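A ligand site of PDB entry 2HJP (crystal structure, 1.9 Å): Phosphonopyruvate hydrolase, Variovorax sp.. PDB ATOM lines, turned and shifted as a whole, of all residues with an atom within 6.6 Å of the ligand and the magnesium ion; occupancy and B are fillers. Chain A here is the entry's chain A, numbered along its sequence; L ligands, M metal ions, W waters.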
ATOM      1  N   ALA A  21      36.745 -10.261 -21.062  1.00  0.00           N
ATOM      2  CA  ALA A  21      36.981  -9.522 -22.280  1.00  0.00           C
ATOM      3  C   ALA A  21      38.465  -9.559 -22.701  1.00  0.00           C
ATOM      4  O   ALA A  21      39.377  -9.581 -21.851  1.00  0.00           O
ATOM      5  CB  ALA A  21      36.579  -8.045 -22.052  1.00  0.00           C
ATOM      6  N   TRP A  40      35.810 -13.410 -23.795  1.00  0.00           N
ATOM      7  CA  TRP A  40      34.683 -12.653 -24.349  1.00  0.00           C
ATOM      8  C   TRP A  40      35.308 -11.772 -25.463  1.00  0.00           C
ATOM      9  O   TRP A  40      36.108 -10.848 -25.181  1.00  0.00           O
ATOM     10  CB  TRP A  40      34.045 -11.793 -23.240  1.00  0.00           C
ATOM     11  CG  TRP A  40      33.111 -10.704 -23.677  1.00  0.00           C
ATOM     12  CD1 TRP A  40      33.143  -9.406 -23.271  1.00  0.00           C
ATOM     13  CD2 TRP A  40      31.969 -10.822 -24.539  1.00  0.00           C
ATOM     14  NE1 TRP A  40      32.086  -8.698 -23.827  1.00  0.00           N
ATOM     15  CE2 TRP A  40      31.356  -9.546 -24.606  1.00  0.00           C
ATOM     16  CE3 TRP A  40      31.394 -11.893 -25.261  1.00  0.00           C
ATOM     17  CZ2 TRP A  40      30.197  -9.294 -25.360  1.00  0.00           C
ATOM     18  CZ3 TRP A  40      30.251 -11.656 -26.014  1.00  0.00           C
ATOM     19  CH2 TRP A  40      29.654 -10.368 -26.066  1.00  0.00           C
ATOM     20  N   GLY A  41      34.949 -12.083 -26.720  1.00  0.00           N
ATOM     21  CA  GLY A  41      35.493 -11.329 -27.858  1.00  0.00           C
ATOM     22  C   GLY A  41      34.639 -10.095 -28.075  1.00  0.00           C
ATOM     23  O   GLY A  41      33.940  -9.925 -29.049  1.00  0.00           O
ATOM     24  N   SER A  42      34.742  -9.219 -27.101  1.00  0.00           N
ATOM     25  CA  SER A  42      34.030  -7.972 -26.992  1.00  0.00           C
ATOM     26  C   SER A  42      34.102  -6.970 -28.182  1.00  0.00           C
ATOM     27  O   SER A  42      35.176  -6.585 -28.565  1.00  0.00           O
ATOM     28  CB  SER A  42      34.591  -7.239 -25.738  1.00  0.00           C
ATOM     29  OG  SER A  42      33.958  -5.962 -25.643  1.00  0.00           O
ATOM     30  N   GLY A  43      32.962  -6.562 -28.727  1.00  0.00           N
ATOM     31  CA  GLY A  43      32.996  -5.534 -29.789  1.00  0.00           C
ATOM     32  C   GLY A  43      33.359  -4.158 -29.187  1.00  0.00           C
ATOM     33  O   GLY A  43      33.967  -3.333 -29.830  1.00  0.00           O
ATOM     34  N   PHE A  44      32.997  -3.918 -27.922  1.00  0.00           N
ATOM     35  CA  PHE A  44      33.279  -2.655 -27.295  1.00  0.00           C
ATOM     36  C   PHE A  44      34.810  -2.542 -27.122  1.00  0.00           C
ATOM     37  O   PHE A  44      35.447  -1.500 -27.458  1.00  0.00           O
ATOM     38  CB  PHE A  44      32.600  -2.605 -25.884  1.00  0.00           C
ATOM     39  CG  PHE A  44      32.942  -1.337 -25.123  1.00  0.00           C
ATOM     40  CD1 PHE A  44      32.276  -0.155 -25.397  1.00  0.00           C
ATOM     41  CD2 PHE A  44      33.988  -1.328 -24.203  1.00  0.00           C
ATOM     42  CE1 PHE A  44      32.660   1.049 -24.744  1.00  0.00           C
ATOM     43  CE2 PHE A  44      34.367  -0.172 -23.568  1.00  0.00           C
ATOM     44  CZ  PHE A  44      33.679   1.047 -23.847  1.00  0.00           C
ATOM     45  N   GLU A  45      35.408  -3.607 -26.590  1.00  0.00           N
ATOM     46  CA  GLU A  45      36.866  -3.605 -26.416  1.00  0.00           C
ATOM     47  C   GLU A  45      37.635  -3.496 -27.728  1.00  0.00           C
ATOM     48  O   GLU A  45      38.577  -2.717 -27.807  1.00  0.00           O
ATOM     49  CB  GLU A  45      37.360  -4.853 -25.722  1.00  0.00           C
ATOM     50  CG  GLU A  45      37.069  -4.818 -24.197  1.00  0.00           C
ATOM     51  CD  GLU A  45      38.274  -5.200 -23.377  1.00  0.00           C
ATOM     52  OE1 GLU A  45      39.264  -5.672 -23.995  1.00  0.00           O
ATOM     53  OE2 GLU A  45      38.229  -5.053 -22.131  1.00  0.00           O
ATOM     54  N   ASP A  54      31.627   2.143 -30.374  1.00  0.00           N
ATOM     55  CA  ASP A  54      31.021   0.808 -30.442  1.00  0.00           C
ATOM     56  C   ASP A  54      29.587   1.048 -31.031  1.00  0.00           C
ATOM     57  O   ASP A  54      28.614   0.936 -30.308  1.00  0.00           O
ATOM     58  CB  ASP A  54      30.961   0.220 -29.015  1.00  0.00           C
ATOM     59  CG  ASP A  54      30.375  -1.206 -28.979  1.00  0.00           C
ATOM     60  OD1 ASP A  54      29.837  -1.614 -27.900  1.00  0.00           O
ATOM     61  OD2 ASP A  54      30.451  -1.897 -30.017  1.00  0.00           O
ATOM     62  N   ASP A  81      31.237 -11.694 -29.797  1.00  0.00           N
ATOM     63  CA  ASP A  81      30.179 -10.691 -29.881  1.00  0.00           C
ATOM     64  C   ASP A  81      29.898 -10.388 -31.386  1.00  0.00           C
ATOM     65  O   ASP A  81      30.768  -9.869 -32.088  1.00  0.00           O
ATOM     66  CB  ASP A  81      30.682  -9.418 -29.186  1.00  0.00           C
ATOM     67  CG  ASP A  81      29.659  -8.297 -29.171  1.00  0.00           C
ATOM     68  OD1 ASP A  81      28.546  -8.416 -29.734  1.00  0.00           O
ATOM     69  OD2 ASP A  81      30.013  -7.251 -28.566  1.00  0.00           O
ATOM     70  N   ASP A  83      27.349  -8.421 -32.435  1.00  0.00           N
ATOM     71  CA  ASP A  83      26.455  -7.261 -32.404  1.00  0.00           C
ATOM     72  C   ASP A  83      25.033  -7.656 -32.811  1.00  0.00           C
ATOM     73  O   ASP A  83      24.446  -8.476 -32.099  1.00  0.00           O
ATOM     74  CB  ASP A  83      26.988  -6.162 -33.334  1.00  0.00           C
ATOM     75  CG  ASP A  83      28.265  -5.432 -32.752  1.00  0.00           C
ATOM     76  OD1 ASP A  83      28.631  -4.374 -33.353  1.00  0.00           O
ATOM     77  OD2 ASP A  83      28.930  -5.886 -31.750  1.00  0.00           O
ATOM     78  N   VAL A 108      27.068 -14.133 -29.513  1.00  0.00           N
ATOM     79  CA  VAL A 108      26.051 -13.370 -28.775  1.00  0.00           C
ATOM     80  C   VAL A 108      25.555 -12.365 -29.839  1.00  0.00           C
ATOM     81  O   VAL A 108      26.334 -11.593 -30.419  1.00  0.00           O
ATOM     82  CB  VAL A 108      26.648 -12.596 -27.571  1.00  0.00           C
ATOM     83  CG1 VAL A 108      25.534 -11.613 -26.922  1.00  0.00           C
ATOM     84  CG2 VAL A 108      27.110 -13.595 -26.544  1.00  0.00           C
ATOM     85  N   GLU A 110      22.323  -9.468 -30.355  1.00  0.00           N
ATOM     86  CA  GLU A 110      21.277  -8.683 -29.638  1.00  0.00           C
ATOM     87  C   GLU A 110      20.126  -8.262 -30.532  1.00  0.00           C
ATOM     88  O   GLU A 110      20.253  -8.192 -31.777  1.00  0.00           O
ATOM     89  CB  GLU A 110      21.923  -7.425 -29.021  1.00  0.00           C
ATOM     90  CG  GLU A 110      22.507  -6.510 -30.125  1.00  0.00           C
ATOM     91  CD  GLU A 110      23.804  -5.802 -29.668  1.00  0.00           C
ATOM     92  OE1 GLU A 110      24.007  -4.660 -30.088  1.00  0.00           O
ATOM     93  OE2 GLU A 110      24.590  -6.385 -28.889  1.00  0.00           O
ATOM     94  N   ARG A 155      20.805 -11.925 -26.935  1.00  0.00           N
ATOM     95  CA  ARG A 155      20.857 -10.843 -25.994  1.00  0.00           C
ATOM     96  C   ARG A 155      19.623  -9.974 -26.091  1.00  0.00           C
ATOM     97  O   ARG A 155      19.267  -9.468 -27.170  1.00  0.00           O
ATOM     98  CB  ARG A 155      22.149 -10.061 -26.208  1.00  0.00           C
ATOM     99  CG  ARG A 155      22.171  -8.681 -25.579  1.00  0.00           C
ATOM    100  CD  ARG A 155      23.593  -8.034 -25.711  1.00  0.00           C
ATOM    101  NE  ARG A 155      23.529  -6.593 -25.543  1.00  0.00           N
ATOM    102  CZ  ARG A 155      24.570  -5.763 -25.381  1.00  0.00           C
ATOM    103  NH1 ARG A 155      25.790  -6.255 -25.325  1.00  0.00           N
ATOM    104  NH2 ARG A 155      24.385  -4.442 -25.315  1.00  0.00           N
ATOM    105  N   GLU A 157      17.698  -6.655 -25.153  1.00  0.00           N
ATOM    106  CA  GLU A 157      17.915  -5.242 -24.857  1.00  0.00           C
ATOM    107  C   GLU A 157      16.686  -4.516 -24.297  1.00  0.00           C
ATOM    108  O   GLU A 157      16.752  -3.310 -23.990  1.00  0.00           O
ATOM    109  CB  GLU A 157      18.317  -4.519 -26.136  1.00  0.00           C
ATOM    110  CG  GLU A 157      19.680  -4.785 -26.663  1.00  0.00           C
ATOM    111  CD  GLU A 157      20.718  -4.146 -25.798  1.00  0.00           C
ATOM    112  OE1 GLU A 157      20.739  -2.902 -25.681  1.00  0.00           O
ATOM    113  OE2 GLU A 157      21.511  -4.899 -25.250  1.00  0.00           O
ATOM    114  N   LEU A 184      21.110 -13.642 -22.712  1.00  0.00           N
ATOM    115  CA  LEU A 184      21.906 -12.659 -22.034  1.00  0.00           C
ATOM    116  C   LEU A 184      20.939 -11.504 -21.828  1.00  0.00           C
ATOM    117  O   LEU A 184      20.461 -10.931 -22.784  1.00  0.00           O
ATOM    118  CB  LEU A 184      23.092 -12.231 -22.924  1.00  0.00           C
ATOM    119  CG  LEU A 184      24.150 -11.348 -22.190  1.00  0.00           C
ATOM    120  CD1 LEU A 184      25.490 -11.281 -23.050  1.00  0.00           C
ATOM    121  CD2 LEU A 184      23.484  -9.934 -21.850  1.00  0.00           C
ATOM    122  N   HIS A 186      20.481  -7.867 -20.451  1.00  0.00           N
ATOM    123  CA  HIS A 186      21.370  -6.765 -20.118  1.00  0.00           C
ATOM    124  C   HIS A 186      20.712  -5.590 -19.360  1.00  0.00           C
ATOM    125  O   HIS A 186      19.494  -5.348 -19.425  1.00  0.00           O
ATOM    126  CB  HIS A 186      22.056  -6.295 -21.401  1.00  0.00           C
ATOM    127  CG  HIS A 186      23.450  -5.759 -21.183  1.00  0.00           C
ATOM    128  ND1 HIS A 186      24.145  -5.894 -19.995  1.00  0.00           N
ATOM    129  CD2 HIS A 186      24.259  -5.028 -22.011  1.00  0.00           C
ATOM    130  CE1 HIS A 186      25.312  -5.274 -20.100  1.00  0.00           C
ATOM    131  NE2 HIS A 186      25.398  -4.740 -21.298  1.00  0.00           N
ATOM    132  N   SER A 187      21.555  -4.872 -18.633  1.00  0.00           N
ATOM    133  CA  SER A 187      21.117  -3.710 -17.853  1.00  0.00           C
ATOM    134  C   SER A 187      22.280  -2.719 -17.663  1.00  0.00           C
ATOM    135  O   SER A 187      23.421  -3.136 -17.495  1.00  0.00           O
ATOM    136  CB  SER A 187      20.601  -4.147 -16.466  1.00  0.00           C
ATOM    137  OG  SER A 187      20.252  -3.005 -15.679  1.00  0.00           O
ATOM    138  N   ARG A 188      21.967  -1.420 -17.734  1.00  0.00           N
ATOM    139  CA  ARG A 188      22.959  -0.360 -17.559  1.00  0.00           C
ATOM    140  C   ARG A 188      22.756   0.336 -16.223  1.00  0.00           C
ATOM    141  O   ARG A 188      23.416   1.371 -15.972  1.00  0.00           O
ATOM    142  CB  ARG A 188      22.815   0.736 -18.612  1.00  0.00           C
ATOM    143  CG  ARG A 188      22.938   0.308 -20.012  1.00  0.00           C
ATOM    144  CD  ARG A 188      24.358   0.115 -20.432  1.00  0.00           C
ATOM    145  NE  ARG A 188      24.316  -0.352 -21.808  1.00  0.00           N
ATOM    146  CZ  ARG A 188      25.307  -1.019 -22.397  1.00  0.00           C
ATOM    147  NH1 ARG A 188      26.428  -1.297 -21.724  1.00  0.00           N
ATOM    148  NH2 ARG A 188      25.142  -1.428 -23.648  1.00  0.00           N
ATOM    149  N   VAL A 211      26.211  -9.548 -17.654  1.00  0.00           N
ATOM    150  CA  VAL A 211      27.411  -8.736 -17.910  1.00  0.00           C
ATOM    151  C   VAL A 211      27.224  -7.621 -16.875  1.00  0.00           C
ATOM    152  O   VAL A 211      26.632  -6.571 -17.172  1.00  0.00           O
ATOM    153  CB  VAL A 211      27.368  -8.145 -19.338  1.00  0.00           C
ATOM    154  CG1 VAL A 211      28.690  -7.358 -19.654  1.00  0.00           C
ATOM    155  CG2 VAL A 211      27.062  -9.281 -20.341  1.00  0.00           C
ATOM    156  N   THR A 213      28.914  -5.259 -15.620  1.00  0.00           N
ATOM    157  CA  THR A 213      29.793  -4.098 -15.731  1.00  0.00           C
ATOM    158  C   THR A 213      29.309  -2.868 -15.044  1.00  0.00           C
ATOM    159  O   THR A 213      30.115  -2.228 -14.353  1.00  0.00           O
ATOM    160  CB  THR A 213      30.052  -3.747 -17.212  1.00  0.00           C
ATOM    161  OG1 THR A 213      30.575  -4.904 -17.842  1.00  0.00           O
ATOM    162  CG2 THR A 213      31.026  -2.560 -17.371  1.00  0.00           C
ATOM    163  N   ILE A 233      29.892 -12.466 -17.656  1.00  0.00           N
ATOM    164  CA  ILE A 233      30.925 -11.935 -18.573  1.00  0.00           C
ATOM    165  C   ILE A 233      31.482 -10.597 -18.011  1.00  0.00           C
ATOM    166  O   ILE A 233      30.688  -9.723 -17.642  1.00  0.00           O
ATOM    167  CB  ILE A 233      30.293 -11.624 -19.977  1.00  0.00           C
ATOM    168  CG1 ILE A 233      30.025 -12.969 -20.723  1.00  0.00           C
ATOM    169  CG2 ILE A 233      31.253 -10.707 -20.853  1.00  0.00           C
ATOM    170  CD1 ILE A 233      31.119 -13.545 -21.598  1.00  0.00           C
ATOM    171  N   TYR A 234      32.812 -10.472 -17.958  1.00  0.00           N
ATOM    172  CA  TYR A 234      33.473  -9.209 -17.556  1.00  0.00           C
ATOM    173  C   TYR A 234      33.654  -8.501 -18.882  1.00  0.00           C
ATOM    174  O   TYR A 234      34.535  -8.817 -19.707  1.00  0.00           O
ATOM    175  CB  TYR A 234      34.722  -9.556 -16.796  1.00  0.00           C
ATOM    176  CG  TYR A 234      34.296 -10.197 -15.480  1.00  0.00           C
ATOM    177  CD1 TYR A 234      33.572  -9.488 -14.546  1.00  0.00           C
ATOM    178  CD2 TYR A 234      34.605 -11.538 -15.198  1.00  0.00           C
ATOM    179  CE1 TYR A 234      33.145 -10.086 -13.335  1.00  0.00           C
ATOM    180  CE2 TYR A 234      34.200 -12.165 -13.994  1.00  0.00           C
ATOM    181  CZ  TYR A 234      33.454 -11.413 -13.077  1.00  0.00           C
ATOM    182  OH  TYR A 234      33.033 -11.998 -11.924  1.00  0.00           O
ATOM    183  N   GLY A 235      32.788  -7.540 -19.089  1.00  0.00           N
ATOM    184  CA  GLY A 235      32.697  -6.919 -20.389  1.00  0.00           C
ATOM    185  C   GLY A 235      33.760  -6.067 -20.974  1.00  0.00           C
ATOM    186  O   GLY A 235      33.952  -6.141 -22.216  1.00  0.00           O
ATOM    187  N   ASN A 236      34.475  -5.296 -20.141  1.00  0.00           N
ATOM    188  CA  ASN A 236      35.483  -4.386 -20.719  1.00  0.00           C
ATOM    189  C   ASN A 236      36.620  -3.992 -19.769  1.00  0.00           C
ATOM    190  O   ASN A 236      37.239  -2.947 -19.934  1.00  0.00           O
ATOM    191  CB  ASN A 236      34.737  -3.088 -21.206  1.00  0.00           C
ATOM    192  CG  ASN A 236      33.899  -2.396 -20.066  1.00  0.00           C
ATOM    193  OD1 ASN A 236      34.181  -2.577 -18.897  1.00  0.00           O
ATOM    194  ND2 ASN A 236      32.853  -1.611 -20.464  1.00  0.00           N
HETATM  195  C1  LIG L   1      30.654  -5.683 -25.480  1.00  0.00           C
HETATM  196  O1  LIG L   1      31.535  -5.959 -24.568  1.00  0.00           O
HETATM  197  O2  LIG L   1      30.907  -5.337 -26.600  1.00  0.00           O
HETATM  198  C2  LIG L   1      29.232  -5.846 -25.031  1.00  0.00           C
HETATM  199  C3  LIG L   1      28.709  -5.648 -23.785  1.00  0.00           C
HETATM  200  O3  LIG L   1      28.421  -6.220 -26.010  1.00  0.00           O
HETATM  201  P1  LIG L   1      28.323  -3.836 -23.605  1.00  0.00           P
HETATM  202  O4  LIG L   1      27.227  -3.579 -24.678  1.00  0.00           O
HETATM  203  O5  LIG L   1      29.653  -3.079 -23.873  1.00  0.00           O
HETATM  204  O6  LIG L   1      27.772  -3.708 -22.261  1.00  0.00           O
HETATM  205 MG    MG M   1      29.192  -5.481 -27.854  1.00  0.00          MG
HETATM  206  O   HOH W   1      26.619  -8.496 -26.549  1.00  0.00           O
HETATM  207  O   HOH W   2      29.914  -4.484 -29.597  1.00  0.00           O
HETATM  208  O   HOH W   3      30.348  -0.870 -22.532  1.00  0.00           O
HETATM  209  O   HOH W   4      27.385  -6.058 -28.809  1.00  0.00           O
HETATM  210  O   HOH W   5      28.417  -3.589 -27.373  1.00  0.00           O
HETATM  211  O   HOH W   6      31.696  -3.870 -22.571  1.00  0.00           O
HETATM  212  O   HOH W   7      27.920  -2.898 -19.300  1.00  0.00           O
HETATM  213  O   HOH W   8      30.169  -4.244 -20.414  1.00  0.00           O
HETATM  214  O   HOH W   9      28.929  -0.738 -25.624  1.00  0.00           O
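The magnesium ion is bound by the side-chain carboxylate (OD2) of Asp 81 (2.1 Å).
Water W5 is bound to the magnesium ion (2.1 Å).
Water W4 is bound to the magnesium ion (2.1 Å).
An oxygen (O2) of the ligand binds the magnesium ion.
The magnesium ion is bound by O3 of the ligand (2.1 Å).
Water W2 binds the magnesium ion (2.1 Å).
The magnesium ion has six donor atoms within binding distance.
An oxygen (O1) of the ligand sits close to the backbone carbonyl oxygen (O) of Gly 235, at 3.4 Å.
Hydrophobic or aromatic side chains that line the ligand: Trp 40, Phe 44 and His 186.
Of the 24 residues printed, 9 come within 4 Å of the ligand.
The nearest printed residue that does not touch the ligand is Asp 54 (4.1 Å).
Merely in contact with the magnesium ion: Asp 54 (3.9 Å) and Asp 83 (3.9 Å).
Three residues have an atom within 4 Å of the magnesium ion: Asp 54, Asp 81 and Asp 83.
Along chain A the residues within 4 Å of the magnesium ion span positions 54 to 83.
An oxygen (O6) of the ligand lies within salt-bridge range of the guanidinium group (NH1) of Arg 188, 2.8 Å away.
An oxygen (O2) of the ligand sits close to the backbone NH (N) of Phe 44 (2.9 Å).
The indole nitrogen (NE1) of Trp 40 lies within hydrogen-bond range of an oxygen (O1) of the ligand, at 2.9 Å.
O1 of the ligand lies within hydrogen-bond range of OG of Ser 42 (2.7 Å).
An oxygen (O4) of the ligand lies within salt-bridge range of the guanidinium group of Arg 155, at 3.0 Å.
The backbone NH (N) of Gly 43 lies close to an oxygen (O2) of the ligand, 3.2 Å away.
An oxygen (O6) of the ligand is in hydrogen-bond range of a ring nitrogen (NE2) of His 186 (2.8 Å).
OD2 of Asp 81 lies close to N of Gly 43.
NE of Arg 155 lies within salt-bridge range of OE2 of Glu 157 (2.7 Å).
The backbone NH (N) of Glu 45 is in hydrogen-bond range of the side-chain hydroxyl (OG) of Ser 42, 2.9 Å away.
NE of Arg 155 is in salt-bridge range of OE2 of Glu 110 (3.5 Å).
N of Asp 81 sits close to O of Gly 41, 3.3 Å away.
The side-chain hydroxyl of Ser 42 lies within hydrogen-bond range of the backbone NH of Phe 44 (3.2 Å).
OG of Ser 42 lies within hydrogen-bond range of O of Gly 235.
N of Glu 110 is in hydrogen-bond range of O of Asp 83.
Water W5 bridges the side-chain carboxylate of Asp 54 and an oxygen (O4) of the ligand.
Water W2 lies within hydrogen-bond range of the side-chain carboxylate of Asp 54 and the side-chain carboxylate of Asp 83.
Water W6 lies within hydrogen-bond range of an oxygen (O5) of the ligand (2.5 Å), the backbone carbonyl oxygen of Gly 235 (3.2 Å) and the side-chain amide nitrogen of Asn 236 (3.3 Å).
Water W3 bridges O5 of the ligand and ND2 of Asn 236.
Water W9 bridges the side-chain carboxylate of Asp 54 (2.6 Å) and an oxygen (O5) of the ligand (3.0 Å).
Water W7 lies within hydrogen-bond range of O6 of the ligand and NH1 of Arg 188.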
